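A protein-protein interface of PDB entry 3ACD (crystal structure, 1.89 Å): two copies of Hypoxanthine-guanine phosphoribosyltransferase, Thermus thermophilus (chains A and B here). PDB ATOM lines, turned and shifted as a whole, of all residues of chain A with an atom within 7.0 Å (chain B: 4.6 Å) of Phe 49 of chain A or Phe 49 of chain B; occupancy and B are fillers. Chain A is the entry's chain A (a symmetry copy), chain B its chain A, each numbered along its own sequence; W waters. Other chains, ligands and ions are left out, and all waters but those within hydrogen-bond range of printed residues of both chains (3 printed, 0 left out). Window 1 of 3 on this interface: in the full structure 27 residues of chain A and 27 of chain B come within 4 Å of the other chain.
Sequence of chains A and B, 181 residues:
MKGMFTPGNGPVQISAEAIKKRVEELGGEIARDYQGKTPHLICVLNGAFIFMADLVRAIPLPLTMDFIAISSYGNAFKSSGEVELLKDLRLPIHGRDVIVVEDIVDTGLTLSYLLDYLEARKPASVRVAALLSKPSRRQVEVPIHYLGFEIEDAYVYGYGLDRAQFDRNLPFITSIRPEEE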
ATOM      1  N   CYS A  43       2.973 -13.335  15.885  1.00  0.00           N
ATOM      2  CA  CYS A  43       2.449 -12.140  15.244  1.00  0.00           C
ATOM      3  C   CYS A  43       1.007 -11.868  15.665  1.00  0.00           C
ATOM      4  O   CYS A  43       0.137 -12.727  15.522  1.00  0.00           O
ATOM      5  CB  CYS A  43       2.512 -12.295  13.725  1.00  0.00           C
ATOM      6  SG  CYS A  43       1.708 -10.952  12.810  1.00  0.00           S
ATOM      7  N   VAL A  44       0.763 -10.672  16.193  1.00  0.00           N
ATOM      8  CA  VAL A  44      -0.583 -10.299  16.600  1.00  0.00           C
ATOM      9  C   VAL A  44      -1.304  -9.709  15.390  1.00  0.00           C
ATOM     10  O   VAL A  44      -1.030  -8.581  14.971  1.00  0.00           O
ATOM     11  CB  VAL A  44      -0.565  -9.264  17.752  1.00  0.00           C
ATOM     12  CG1 VAL A  44      -1.990  -8.851  18.110  1.00  0.00           C
ATOM     13  CG2 VAL A  44       0.119  -9.862  18.978  1.00  0.00           C
ATOM     14  N   LEU A  45      -2.218 -10.488  14.820  1.00  0.00           N
ATOM     15  CA  LEU A  45      -2.991 -10.066  13.652  1.00  0.00           C
ATOM     16  C   LEU A  45      -4.084  -9.079  14.060  1.00  0.00           C
ATOM     17  O   LEU A  45      -4.525  -9.091  15.208  1.00  0.00           O
ATOM     18  CB  LEU A  45      -3.628 -11.290  12.983  1.00  0.00           C
ATOM     19  CG  LEU A  45      -2.665 -12.284  12.330  1.00  0.00           C
ATOM     20  CD1 LEU A  45      -3.425 -13.525  11.882  1.00  0.00           C
ATOM     21  CD2 LEU A  45      -1.979 -11.615  11.147  1.00  0.00           C
ATOM     22  N   ASN A  46      -4.544  -8.244  13.132  1.00  0.00           N
ATOM     23  CA  ASN A  46      -4.077  -8.216  11.743  1.00  0.00           C
ATOM     24  C   ASN A  46      -2.968  -7.191  11.511  1.00  0.00           C
ATOM     25  O   ASN A  46      -2.140  -7.353  10.615  1.00  0.00           O
ATOM     26  CB  ASN A  46      -5.235  -7.846  10.803  1.00  0.00           C
ATOM     27  CG  ASN A  46      -6.300  -8.923  10.712  1.00  0.00           C
ATOM     28  OD1 ASN A  46      -7.390  -8.683  10.188  1.00  0.00           O
ATOM     29  ND2 ASN A  46      -5.991 -10.112  11.199  1.00  0.00           N
ATOM     30  N   GLY A  47      -2.969  -6.139  12.321  1.00  0.00           N
ATOM     31  CA  GLY A  47      -2.016  -5.049  12.165  1.00  0.00           C
ATOM     32  C   GLY A  47      -0.515  -5.268  12.086  1.00  0.00           C
ATOM     33  O   GLY A  47       0.179  -4.499  11.420  1.00  0.00           O
ATOM     34  N   ALA A  48       0.003  -6.295  12.744  1.00  0.00           N
ATOM     35  CA  ALA A  48       1.446  -6.515  12.740  1.00  0.00           C
ATOM     36  C   ALA A  48       2.007  -7.405  11.639  1.00  0.00           C
ATOM     37  O   ALA A  48       3.212  -7.645  11.606  1.00  0.00           O
ATOM     38  CB  ALA A  48       1.873  -7.067  14.103  1.00  0.00           C
ATOM     39  N   PHE A  49       1.173  -7.871  10.716  1.00  0.00           N
ATOM     40  CA  PHE A  49       1.690  -8.796   9.713  1.00  0.00           C
ATOM     41  C   PHE A  49       2.788  -8.295   8.774  1.00  0.00           C
ATOM     42  O   PHE A  49       3.637  -9.086   8.358  1.00  0.00           O
ATOM     43  CB  PHE A  49       0.527  -9.436   8.928  1.00  0.00           C
ATOM     44  CG  PHE A  49       0.133  -8.703   7.679  1.00  0.00           C
ATOM     45  CD1 PHE A  49       0.600  -9.130   6.438  1.00  0.00           C
ATOM     46  CD2 PHE A  49      -0.748  -7.629   7.731  1.00  0.00           C
ATOM     47  CE1 PHE A  49       0.187  -8.502   5.263  1.00  0.00           C
ATOM     48  CE2 PHE A  49      -1.170  -6.989   6.556  1.00  0.00           C
ATOM     49  CZ  PHE A  49      -0.701  -7.431   5.323  1.00  0.00           C
ATOM     50  N   ILE A  50       2.801  -7.003   8.449  1.00  0.00           N
ATOM     51  CA  ILE A  50       3.845  -6.479   7.568  1.00  0.00           C
ATOM     52  C   ILE A  50       5.132  -6.275   8.372  1.00  0.00           C
ATOM     53  O   ILE A  50       6.227  -6.610   7.909  1.00  0.00           O
ATOM     54  CB  ILE A  50       3.378  -5.166   6.873  1.00  0.00           C
ATOM     55  CG1 ILE A  50       2.193  -5.495   5.950  1.00  0.00           C
ATOM     56  CG2 ILE A  50       4.522  -4.549   6.073  1.00  0.00           C
ATOM     57  CD1 ILE A  50       1.741  -4.367   5.031  1.00  0.00           C
ATOM     58  N   PHE A  51       4.997  -5.735   9.580  1.00  0.00           N
ATOM     59  CA  PHE A  51       6.136  -5.544  10.472  1.00  0.00           C
ATOM     60  C   PHE A  51       6.770  -6.923  10.685  1.00  0.00           C
ATOM     61  O   PHE A  51       7.992  -7.085  10.622  1.00  0.00           O
ATOM     62  CB  PHE A  51       5.643  -4.959  11.800  1.00  0.00           C
ATOM     63  CG  PHE A  51       6.695  -4.880  12.878  1.00  0.00           C
ATOM     64  CD1 PHE A  51       7.973  -4.409  12.603  1.00  0.00           C
ATOM     65  CD2 PHE A  51       6.377  -5.220  14.193  1.00  0.00           C
ATOM     66  CE1 PHE A  51       8.922  -4.270  13.624  1.00  0.00           C
ATOM     67  CE2 PHE A  51       7.318  -5.086  15.218  1.00  0.00           C
ATOM     68  CZ  PHE A  51       8.594  -4.608  14.931  1.00  0.00           C
ATOM     69  N   MET A  52       5.926  -7.923  10.925  1.00  0.00           N
ATOM     70  CA  MET A  52       6.388  -9.296  11.125  1.00  0.00           C
ATOM     71  C   MET A  52       7.151  -9.802   9.896  1.00  0.00           C
ATOM     72  O   MET A  52       8.259 -10.338  10.012  1.00  0.00           O
ATOM     73  CB  MET A  52       5.186 -10.208  11.390  1.00  0.00           C
ATOM     74  CG  MET A  52       5.537 -11.681  11.556  1.00  0.00           C
ATOM     75  SD  MET A  52       6.128 -12.111  13.208  1.00  0.00           S
ATOM     76  CE  MET A  52       5.897 -13.911  13.174  1.00  0.00           C
ATOM     77  N   ALA A  53       6.557  -9.638   8.716  1.00  0.00           N
ATOM     78  CA  ALA A  53       7.184 -10.093   7.476  1.00  0.00           C
ATOM     79  C   ALA A  53       8.571  -9.489   7.266  1.00  0.00           C
ATOM     80  O   ALA A  53       9.504 -10.189   6.877  1.00  0.00           O
ATOM     81  CB  ALA A  53       6.288  -9.761   6.277  1.00  0.00           C
ATOM     82  N   ASP A  54       8.712  -8.193   7.528  1.00  0.00           N
ATOM     83  CA  ASP A  54      10.008  -7.542   7.350  1.00  0.00           C
ATOM     84  C   ASP A  54      10.988  -7.890   8.467  1.00  0.00           C
ATOM     85  O   ASP A  54      12.171  -8.117   8.218  1.00  0.00           O
ATOM     86  CB  ASP A  54       9.838  -6.022   7.278  1.00  0.00           C
ATOM     87  CG  ASP A  54       9.101  -5.575   6.032  1.00  0.00           C
ATOM     88  OD1 ASP A  54       8.820  -6.429   5.165  1.00  0.00           O
ATOM     89  OD2 ASP A  54       8.806  -4.369   5.916  1.00  0.00           O
ATOM     90  N   VAL A  56      11.181 -10.677  10.525  1.00  0.00           N
ATOM     91  CA  VAL A  56      11.748 -12.020  10.499  1.00  0.00           C
ATOM     92  C   VAL A  56      12.835 -12.178   9.440  1.00  0.00           C
ATOM     93  O   VAL A  56      13.808 -12.905   9.647  1.00  0.00           O
ATOM     94  CB  VAL A  56      10.658 -13.115  10.314  1.00  0.00           C
ATOM     95  CG1 VAL A  56       9.659 -13.040  11.468  1.00  0.00           C
ATOM     96  CG2 VAL A  56       9.952 -12.964   8.970  1.00  0.00           C
ATOM     97  N   ARG A  57      12.688 -11.482   8.318  1.00  0.00           N
ATOM     98  CA  ARG A  57      13.682 -11.557   7.256  1.00  0.00           C
ATOM     99  C   ARG A  57      14.975 -10.845   7.635  1.00  0.00           C
ATOM    100  O   ARG A  57      15.953 -10.883   6.887  1.00  0.00           O
ATOM    101  CB  ARG A  57      13.119 -10.977   5.958  1.00  0.00           C
ATOM    102  CG  ARG A  57      12.153 -11.924   5.258  1.00  0.00           C
ATOM    103  CD  ARG A  57      11.609 -11.330   3.973  1.00  0.00           C
ATOM    104  NE  ARG A  57      10.607 -10.294   4.217  1.00  0.00           N
ATOM    105  CZ  ARG A  57       9.916  -9.696   3.250  1.00  0.00           C
ATOM    106  NH1 ARG A  57      10.133 -10.039   1.985  1.00  0.00           N
ATOM    107  NH2 ARG A  57       9.004  -8.772   3.542  1.00  0.00           N
ATOM    108  N   MET A  65       7.195 -19.645  14.042  1.00  0.00           N
ATOM    109  CA  MET A  65       6.230 -18.559  14.121  1.00  0.00           C
ATOM    110  C   MET A  65       4.815 -19.060  14.340  1.00  0.00           C
ATOM    111  O   MET A  65       4.501 -20.227  14.100  1.00  0.00           O
ATOM    112  CB  MET A  65       6.226 -17.755  12.812  1.00  0.00           C
ATOM    113  CG  MET A  65       7.587 -17.308  12.286  1.00  0.00           C
ATOM    114  SD  MET A  65       7.386 -16.532  10.645  1.00  0.00           S
ATOM    115  CE  MET A  65       9.108 -16.429  10.091  1.00  0.00           C
ATOM    116  N   PHE A  67       0.508 -17.185  14.664  1.00  0.00           N
ATOM    117  CA  PHE A  67      -0.317 -15.996  14.503  1.00  0.00           C
ATOM    118  C   PHE A  67      -1.518 -16.078  15.431  1.00  0.00           C
ATOM    119  O   PHE A  67      -2.112 -17.143  15.599  1.00  0.00           O
ATOM    120  CB  PHE A  67      -0.789 -15.891  13.051  1.00  0.00           C
ATOM    121  CG  PHE A  67       0.325 -15.684  12.068  1.00  0.00           C
ATOM    122  CD1 PHE A  67       0.657 -14.405  11.631  1.00  0.00           C
ATOM    123  CD2 PHE A  67       1.076 -16.763  11.611  1.00  0.00           C
ATOM    124  CE1 PHE A  67       1.720 -14.201  10.754  1.00  0.00           C
ATOM    125  CE2 PHE A  67       2.144 -16.570  10.735  1.00  0.00           C
ATOM    126  CZ  PHE A  67       2.466 -15.288  10.306  1.00  0.00           C
ATOM    127  N   VAL A 101       5.083 -10.045  18.566  1.00  0.00           N
ATOM    128  CA  VAL A 101       5.283  -9.012  17.557  1.00  0.00           C
ATOM    129  C   VAL A 101       3.974  -8.241  17.387  1.00  0.00           C
ATOM    130  O   VAL A 101       2.994  -8.760  16.844  1.00  0.00           O
ATOM    131  CB  VAL A 101       5.724  -9.623  16.206  1.00  0.00           C
ATOM    132  CG1 VAL A 101       5.949  -8.517  15.181  1.00  0.00           C
ATOM    133  CG2 VAL A 101       7.007 -10.431  16.399  1.00  0.00           C
ATOM    134  N   ASP A 103       1.863  -4.362  16.456  1.00  0.00           N
ATOM    135  CA  ASP A 103       1.923  -3.226  15.549  1.00  0.00           C
ATOM    136  C   ASP A 103       2.168  -1.940  16.327  1.00  0.00           C
ATOM    137  O   ASP A 103       3.165  -1.250  16.101  1.00  0.00           O
ATOM    138  CB  ASP A 103       0.638  -3.108  14.702  1.00  0.00           C
ATOM    139  CG  ASP A 103      -0.650  -3.102  15.534  1.00  0.00           C
ATOM    140  OD1 ASP A 103      -0.609  -3.300  16.769  1.00  0.00           O
ATOM    141  OD2 ASP A 103      -1.728  -2.898  14.929  1.00  0.00           O
ATOM    142  N   TYR A 159       1.334   0.528   6.521  1.00  0.00           N
ATOM    143  CA  TYR A 159       2.286  -0.512   6.905  1.00  0.00           C
ATOM    144  C   TYR A 159       1.612  -1.576   7.789  1.00  0.00           C
ATOM    145  O   TYR A 159       2.143  -1.959   8.834  1.00  0.00           O
ATOM    146  CB  TYR A 159       3.471   0.126   7.651  1.00  0.00           C
ATOM    147  CG  TYR A 159       4.698  -0.761   7.789  1.00  0.00           C
ATOM    148  CD1 TYR A 159       5.572  -0.961   6.716  1.00  0.00           C
ATOM    149  CD2 TYR A 159       4.978  -1.405   8.993  1.00  0.00           C
ATOM    150  CE1 TYR A 159       6.701  -1.785   6.845  1.00  0.00           C
ATOM    151  CE2 TYR A 159       6.092  -2.228   9.132  1.00  0.00           C
ATOM    152  CZ  TYR A 159       6.949  -2.416   8.059  1.00  0.00           C
ATOM    153  OH  TYR A 159       8.038  -3.248   8.209  1.00  0.00           O
ATOM    154  N   GLY A 160       0.438  -2.037   7.366  1.00  0.00           N
ATOM    155  CA  GLY A 160      -0.275  -3.056   8.122  1.00  0.00           C
ATOM    156  C   GLY A 160      -1.395  -2.537   9.008  1.00  0.00           C
ATOM    157  O   GLY A 160      -2.387  -3.234   9.239  1.00  0.00           O
ATOM    158  N   LEU A 161      -1.241  -1.314   9.508  1.00  0.00           N
ATOM    159  CA  LEU A 161      -2.246  -0.716  10.378  1.00  0.00           C
ATOM    160  C   LEU A 161      -3.364  -0.122   9.532  1.00  0.00           C
ATOM    161  O   LEU A 161      -3.114   0.524   8.514  1.00  0.00           O
ATOM    162  CB  LEU A 161      -1.612   0.358  11.270  1.00  0.00           C
ATOM    163  CG  LEU A 161      -0.661  -0.146  12.369  1.00  0.00           C
ATOM    164  CD1 LEU A 161       0.558  -0.805  11.745  1.00  0.00           C
ATOM    165  CD2 LEU A 161      -0.229   1.020  13.252  1.00  0.00           C
ATOM    166  N   ARG A 168      -4.052  -0.488   4.943  1.00  0.00           N
ATOM    167  CA  ARG A 168      -3.020  -1.347   5.520  1.00  0.00           C
ATOM    168  C   ARG A 168      -1.898  -1.512   4.491  1.00  0.00           C
ATOM    169  O   ARG A 168      -0.765  -1.827   4.846  1.00  0.00           O
ATOM    170  CB  ARG A 168      -3.573  -2.742   5.847  1.00  0.00           C
ATOM    171  CG  ARG A 168      -4.629  -2.819   6.949  1.00  0.00           C
ATOM    172  CD  ARG A 168      -4.985  -4.288   7.197  1.00  0.00           C
ATOM    173  NE  ARG A 168      -6.154  -4.471   8.055  1.00  0.00           N
ATOM    174  CZ  ARG A 168      -6.155  -4.339   9.378  1.00  0.00           C
ATOM    175  NH1 ARG A 168      -5.041  -4.021  10.026  1.00  0.00           N
ATOM    176  NH2 ARG A 168      -7.282  -4.533  10.055  1.00  0.00           N
ATOM    177  N   ASN A 169      -2.221  -1.285   3.218  1.00  0.00           N
ATOM    178  CA  ASN A 169      -1.250  -1.454   2.142  1.00  0.00           C
ATOM    179  C   ASN A 169      -0.273  -0.307   1.880  1.00  0.00           C
ATOM    180  O   ASN A 169       0.614  -0.435   1.039  1.00  0.00           O
ATOM    181  CB  ASN A 169      -1.980  -1.838   0.842  1.00  0.00           C
ATOM    182  CG  ASN A 169      -3.015  -0.806   0.414  1.00  0.00           C
ATOM    183  OD1 ASN A 169      -3.754  -0.266   1.238  1.00  0.00           O
ATOM    184  ND2 ASN A 169      -3.087  -0.552  -0.886  1.00  0.00           N
ATOM    185  N   CYS B  43      -5.488 -13.455   2.649  1.00  0.00           N
ATOM    186  CA  CYS B  43      -4.225 -14.154   2.813  1.00  0.00           C
ATOM    187  C   CYS B  43      -4.423 -15.524   3.450  1.00  0.00           C
ATOM    188  O   CYS B  43      -5.005 -15.639   4.531  1.00  0.00           O
ATOM    189  CB  CYS B  43      -3.280 -13.323   3.681  1.00  0.00           C
ATOM    190  SG  CYS B  43      -1.740 -14.173   4.121  1.00  0.00           S
ATOM    191  N   LEU B  45      -3.081 -18.166   5.510  1.00  0.00           N
ATOM    192  CA  LEU B  45      -2.024 -18.398   6.495  1.00  0.00           C
ATOM    193  C   LEU B  45      -1.676 -19.885   6.567  1.00  0.00           C
ATOM    194  O   LEU B  45      -2.510 -20.728   6.243  1.00  0.00           O
ATOM    195  CB  LEU B  45      -2.487 -17.911   7.873  1.00  0.00           C
ATOM    196  CG  LEU B  45      -2.679 -16.402   8.030  1.00  0.00           C
ATOM    197  CD1 LEU B  45      -3.316 -16.097   9.378  1.00  0.00           C
ATOM    198  CD2 LEU B  45      -1.331 -15.708   7.900  1.00  0.00           C
ATOM    199  N   ASN B  46      -0.466 -20.218   7.012  1.00  0.00           N
ATOM    200  CA  ASN B  46       0.548 -19.253   7.446  1.00  0.00           C
ATOM    201  C   ASN B  46       1.524 -18.880   6.332  1.00  0.00           C
ATOM    202  O   ASN B  46       2.088 -17.785   6.330  1.00  0.00           O
ATOM    203  CB  ASN B  46       1.380 -19.841   8.595  1.00  0.00           C
ATOM    204  CG  ASN B  46       0.594 -20.005   9.882  1.00  0.00           C
ATOM    205  OD1 ASN B  46       1.049 -20.669  10.815  1.00  0.00           O
ATOM    206  ND2 ASN B  46      -0.576 -19.394   9.949  1.00  0.00           N
ATOM    207  N   GLY B  47       1.720 -19.802   5.396  1.00  0.00           N
ATOM    208  CA  GLY B  47       2.680 -19.610   4.317  1.00  0.00           C
ATOM    209  C   GLY B  47       2.685 -18.381   3.424  1.00  0.00           C
ATOM    210  O   GLY B  47       3.748 -17.972   2.956  1.00  0.00           O
ATOM    211  N   ALA B  48       1.530 -17.781   3.177  1.00  0.00           N
ATOM    212  CA  ALA B  48       1.477 -16.629   2.283  1.00  0.00           C
ATOM    213  C   ALA B  48       1.639 -15.253   2.918  1.00  0.00           C
ATOM    214  O   ALA B  48       1.577 -14.248   2.213  1.00  0.00           O
ATOM    215  CB  ALA B  48       0.169 -16.667   1.490  1.00  0.00           C
ATOM    216  N   PHE B  49       1.884 -15.183   4.222  1.00  0.00           N
ATOM    217  CA  PHE B  49       1.950 -13.867   4.849  1.00  0.00           C
ATOM    218  C   PHE B  49       3.039 -12.902   4.377  1.00  0.00           C
ATOM    219  O   PHE B  49       2.819 -11.690   4.387  1.00  0.00           O
ATOM    220  CB  PHE B  49       1.949 -14.007   6.384  1.00  0.00           C
ATOM    221  CG  PHE B  49       3.312 -14.090   7.009  1.00  0.00           C
ATOM    222  CD1 PHE B  49       3.897 -12.958   7.570  1.00  0.00           C
ATOM    223  CD2 PHE B  49       3.983 -15.304   7.092  1.00  0.00           C
ATOM    224  CE1 PHE B  49       5.132 -13.036   8.215  1.00  0.00           C
ATOM    225  CE2 PHE B  49       5.227 -15.394   7.737  1.00  0.00           C
ATOM    226  CZ  PHE B  49       5.796 -14.256   8.300  1.00  0.00           C
ATOM    227  N   ILE B  50       4.192 -13.411   3.948  1.00  0.00           N
ATOM    228  CA  ILE B  50       5.253 -12.526   3.471  1.00  0.00           C
ATOM    229  C   ILE B  50       4.937 -12.079   2.041  1.00  0.00           C
ATOM    230  O   ILE B  50       5.095 -10.904   1.694  1.00  0.00           O
ATOM    231  CB  ILE B  50       6.644 -13.218   3.570  1.00  0.00           C
ATOM    232  CG1 ILE B  50       6.961 -13.471   5.053  1.00  0.00           C
ATOM    233  CG2 ILE B  50       7.724 -12.345   2.935  1.00  0.00           C
ATOM    234  CD1 ILE B  50       8.375 -13.955   5.351  1.00  0.00           C
ATOM    235  N   PHE B  51       4.479 -13.016   1.216  1.00  0.00           N
ATOM    236  CA  PHE B  51       4.082 -12.710  -0.156  1.00  0.00           C
ATOM    237  C   PHE B  51       2.988 -11.637  -0.072  1.00  0.00           C
ATOM    238  O   PHE B  51       3.003 -10.647  -0.807  1.00  0.00           O
ATOM    239  CB  PHE B  51       3.547 -13.983  -0.821  1.00  0.00           C
ATOM    240  CG  PHE B  51       2.933 -13.768  -2.181  1.00  0.00           C
ATOM    241  CD1 PHE B  51       3.555 -12.967  -3.133  1.00  0.00           C
ATOM    242  CD2 PHE B  51       1.757 -14.429  -2.532  1.00  0.00           C
ATOM    243  CE1 PHE B  51       3.017 -12.829  -4.418  1.00  0.00           C
ATOM    244  CE2 PHE B  51       1.212 -14.299  -3.813  1.00  0.00           C
ATOM    245  CZ  PHE B  51       1.846 -13.497  -4.758  1.00  0.00           C
ATOM    246  N   MET B  52       2.044 -11.838   0.842  1.00  0.00           N
ATOM    247  CA  MET B  52       0.952 -10.888   1.048  1.00  0.00           C
ATOM    248  C   MET B  52       1.494  -9.506   1.436  1.00  0.00           C
ATOM    249  O   MET B  52       1.108  -8.487   0.853  1.00  0.00           O
ATOM    250  CB  MET B  52       0.027 -11.400   2.157  1.00  0.00           C
ATOM    251  CG  MET B  52      -1.121 -10.462   2.505  1.00  0.00           C
ATOM    252  SD  MET B  52      -2.530 -10.581   1.381  1.00  0.00           S
ATOM    253  CE  MET B  52      -3.818  -9.797   2.394  1.00  0.00           C
ATOM    254  N   ALA B  53       2.385  -9.472   2.425  1.00  0.00           N
ATOM    255  CA  ALA B  53       2.961  -8.210   2.887  1.00  0.00           C
ATOM    256  C   ALA B  53       3.639  -7.429   1.764  1.00  0.00           C
ATOM    257  O   ALA B  53       3.473  -6.214   1.659  1.00  0.00           O
ATOM    258  CB  ALA B  53       3.964  -8.470   4.017  1.00  0.00           C
ATOM    259  N   VAL B  56       0.719  -6.449  -1.294  1.00  0.00           N
ATOM    260  CA  VAL B  56      -0.187  -5.333  -1.050  1.00  0.00           C
ATOM    261  C   VAL B  56       0.510  -3.978  -1.141  1.00  0.00           C
ATOM    262  O   VAL B  56      -0.085  -3.000  -1.593  1.00  0.00           O
ATOM    263  CB  VAL B  56      -0.924  -5.464   0.315  1.00  0.00           C
ATOM    264  CG1 VAL B  56      -1.741  -6.754   0.332  1.00  0.00           C
ATOM    265  CG2 VAL B  56       0.064  -5.425   1.477  1.00  0.00           C
ATOM    266  N   MET B  65      -8.444  -6.294   3.675  1.00  0.00           N
ATOM    267  CA  MET B  65      -7.788  -7.588   3.796  1.00  0.00           C
ATOM    268  C   MET B  65      -8.401  -8.447   4.885  1.00  0.00           C
ATOM    269  O   MET B  65      -9.097  -7.957   5.776  1.00  0.00           O
ATOM    270  CB  MET B  65      -6.304  -7.401   4.149  1.00  0.00           C
ATOM    271  CG  MET B  65      -5.522  -6.410   3.292  1.00  0.00           C
ATOM    272  SD  MET B  65      -3.844  -6.196   3.979  1.00  0.00           S
ATOM    273  CE  MET B  65      -3.263  -4.755   3.047  1.00  0.00           C
ATOM    274  N   PHE B  67      -7.588 -12.664   6.815  1.00  0.00           N
ATOM    275  CA  PHE B  67      -6.682 -13.798   6.924  1.00  0.00           C
ATOM    276  C   PHE B  67      -7.468 -15.050   7.279  1.00  0.00           C
ATOM    277  O   PHE B  67      -8.393 -15.001   8.092  1.00  0.00           O
ATOM    278  CB  PHE B  67      -5.635 -13.518   8.006  1.00  0.00           C
ATOM    279  CG  PHE B  67      -4.727 -12.368   7.683  1.00  0.00           C
ATOM    280  CD1 PHE B  67      -3.482 -12.591   7.103  1.00  0.00           C
ATOM    281  CD2 PHE B  67      -5.132 -11.059   7.917  1.00  0.00           C
ATOM    282  CE1 PHE B  67      -2.653 -11.526   6.758  1.00  0.00           C
ATOM    283  CE2 PHE B  67      -4.310  -9.985   7.574  1.00  0.00           C
ATOM    284  CZ  PHE B  67      -3.070 -10.220   6.993  1.00  0.00           C
ATOM    285  N   GLY B 160       8.340 -17.181   3.880  1.00  0.00           N
ATOM    286  CA  GLY B 160       7.034 -17.517   4.426  1.00  0.00           C
ATOM    287  C   GLY B 160       6.713 -19.001   4.470  1.00  0.00           C
ATOM    288  O   GLY B 160       5.981 -19.459   5.352  1.00  0.00           O
HETATM  289  O   HOH W   1       3.288 -21.787  12.271  1.00  0.00           O
HETATM  290  O   HOH W   2      -9.039  -7.171   8.351  1.00  0.00           O
HETATM  291  O   HOH W   3      -8.337  -4.783   6.163  1.00  0.00           O
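Hydrophobic or aromatic side chains of chain B within 4 Å of the printed part of chain A: Leu 45, Phe 49, Ile 50, Met 52, Ala 53, Val 56, Met 65 and Phe 67. Among the printed residues, 19 pairs touch across the chains. Among the printed residues, no Asp or Glu carboxylate lies within 4 Å of a Lys or Arg side-chain nitrogen of the other chain.
Of chain B, only Phe 49, Met 52, Ala 53, Met 65 and Phe 67 come within 4 Å of Phe 49 of chain A. Of chain A, only Phe 49 (3.96 Å), Met 52 (3.6 Å), Ala 53 (3.7 Å), Met 65 (3.6 Å) and Phe 67 (3.6 Å) come within 4 Å of Phe 49 of chain B. Of the printed residues of chain B, Asn 46 of chain A touches Phe 67 (3.5 Å). Of the printed residues of chain A, Met 52 of chain B touches Phe 49 (3.6 Å). Printed residues of chain A within 4 Å of Phe 67 of chain B: Asn 46 (3.5 Å) and Phe 49 (3.6 Å). Of the printed residues of chain B, Met 52 of chain A touches Phe 49 (3.6 Å). Of the printed residues of chain A, Val 56 of chain B touches Asn 169 (3.3 Å). Tyr 159 of chain A touches none of the printed residues of chain B.
Water W2 lies within hydrogen-bond range of O of Met 65 of chain B (2.7 Å) and OD1 of Asn 46 of chain A (2.9 Å). Water W1 bridges the backbone carbonyl oxygen of Met 65 of chain A (2.7 Å) and the side-chain amide oxygen of Asn 46 of chain B (2.9 Å). Water W3 lies within hydrogen-bond range of the guanidinium group (NE) of Arg 168 of chain A (2.9 Å) and the backbone NH (N) of Met 65 of chain B (2.9 Å).
Asn 46 of chain A touches Phe 67 of chain B, and with the chains exchanged Phe 67 of chain A touches Asn 46 of chain B. Phe 49 of chain A touches Met 52 of chain B, and with the chains exchanged Met 52 of chain A touches Phe 49 of chain B. Phe 49 of chain A touches Ala 53 of chain B, and with the chains exchanged Ala 53 of chain A touches Phe 49 of chain B. Ala 53 of chain A touches its own counterpart, Ala 53 of chain B. Positions printed for both chains: 43, 45, 46, 47, 48, 49, 50, 51, 52, 53, 56, 65, 67 and 160.
ND2 of Asn 46 of chain A touches CD2 of Phe 67 of chain B, 3.5 Å away. Phe 49 of chain A touches Met 52 of chain B. CE1 of Phe 49 of chain A touches CA of Ala 53 of chain B (3.7 Å). Phe 49 of chain A touches Met 65 of chain B (CZ to SD, 3.6 Å). Phe 49 of chain A touches Phe 67 of chain B. Ile 50 of chain A touches Ala 53 of chain B (CG1 to CB, 3.97 Å). Met 52 of chain A touches Phe 49 of chain B. CZ of Arg 57 of chain A touches CG2 of Ile 50 of chain B (3.5 Å). Arg 168 of chain A touches Met 65 of chain B. N of Asn 169 of chain A touches CE of Met 65 of chain B, 3.6 Å away.
SG of Cys 43 of chain B sits at hydrogen-bond distance from N of Phe 49 of chain B (3.8 Å). SG of Cys 43 of chain A is in hydrogen-bond range of N of Phe 49 of chain A (3.8 Å). NE of Arg 57 of chain A is in hydrogen-bond range of O of Ala 53 of chain A (2.9 Å). The guanidinium group of Arg 57 of chain A lies within salt-bridge range of the side-chain carboxylate of Asp 54 of chain A, at 2.9 Å. The backbone carbonyl oxygen (O) of Arg 168 of chain A lies within hydrogen-bond range of the backbone NH (N) of Gly 160 of chain A, 2.8 Å away.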
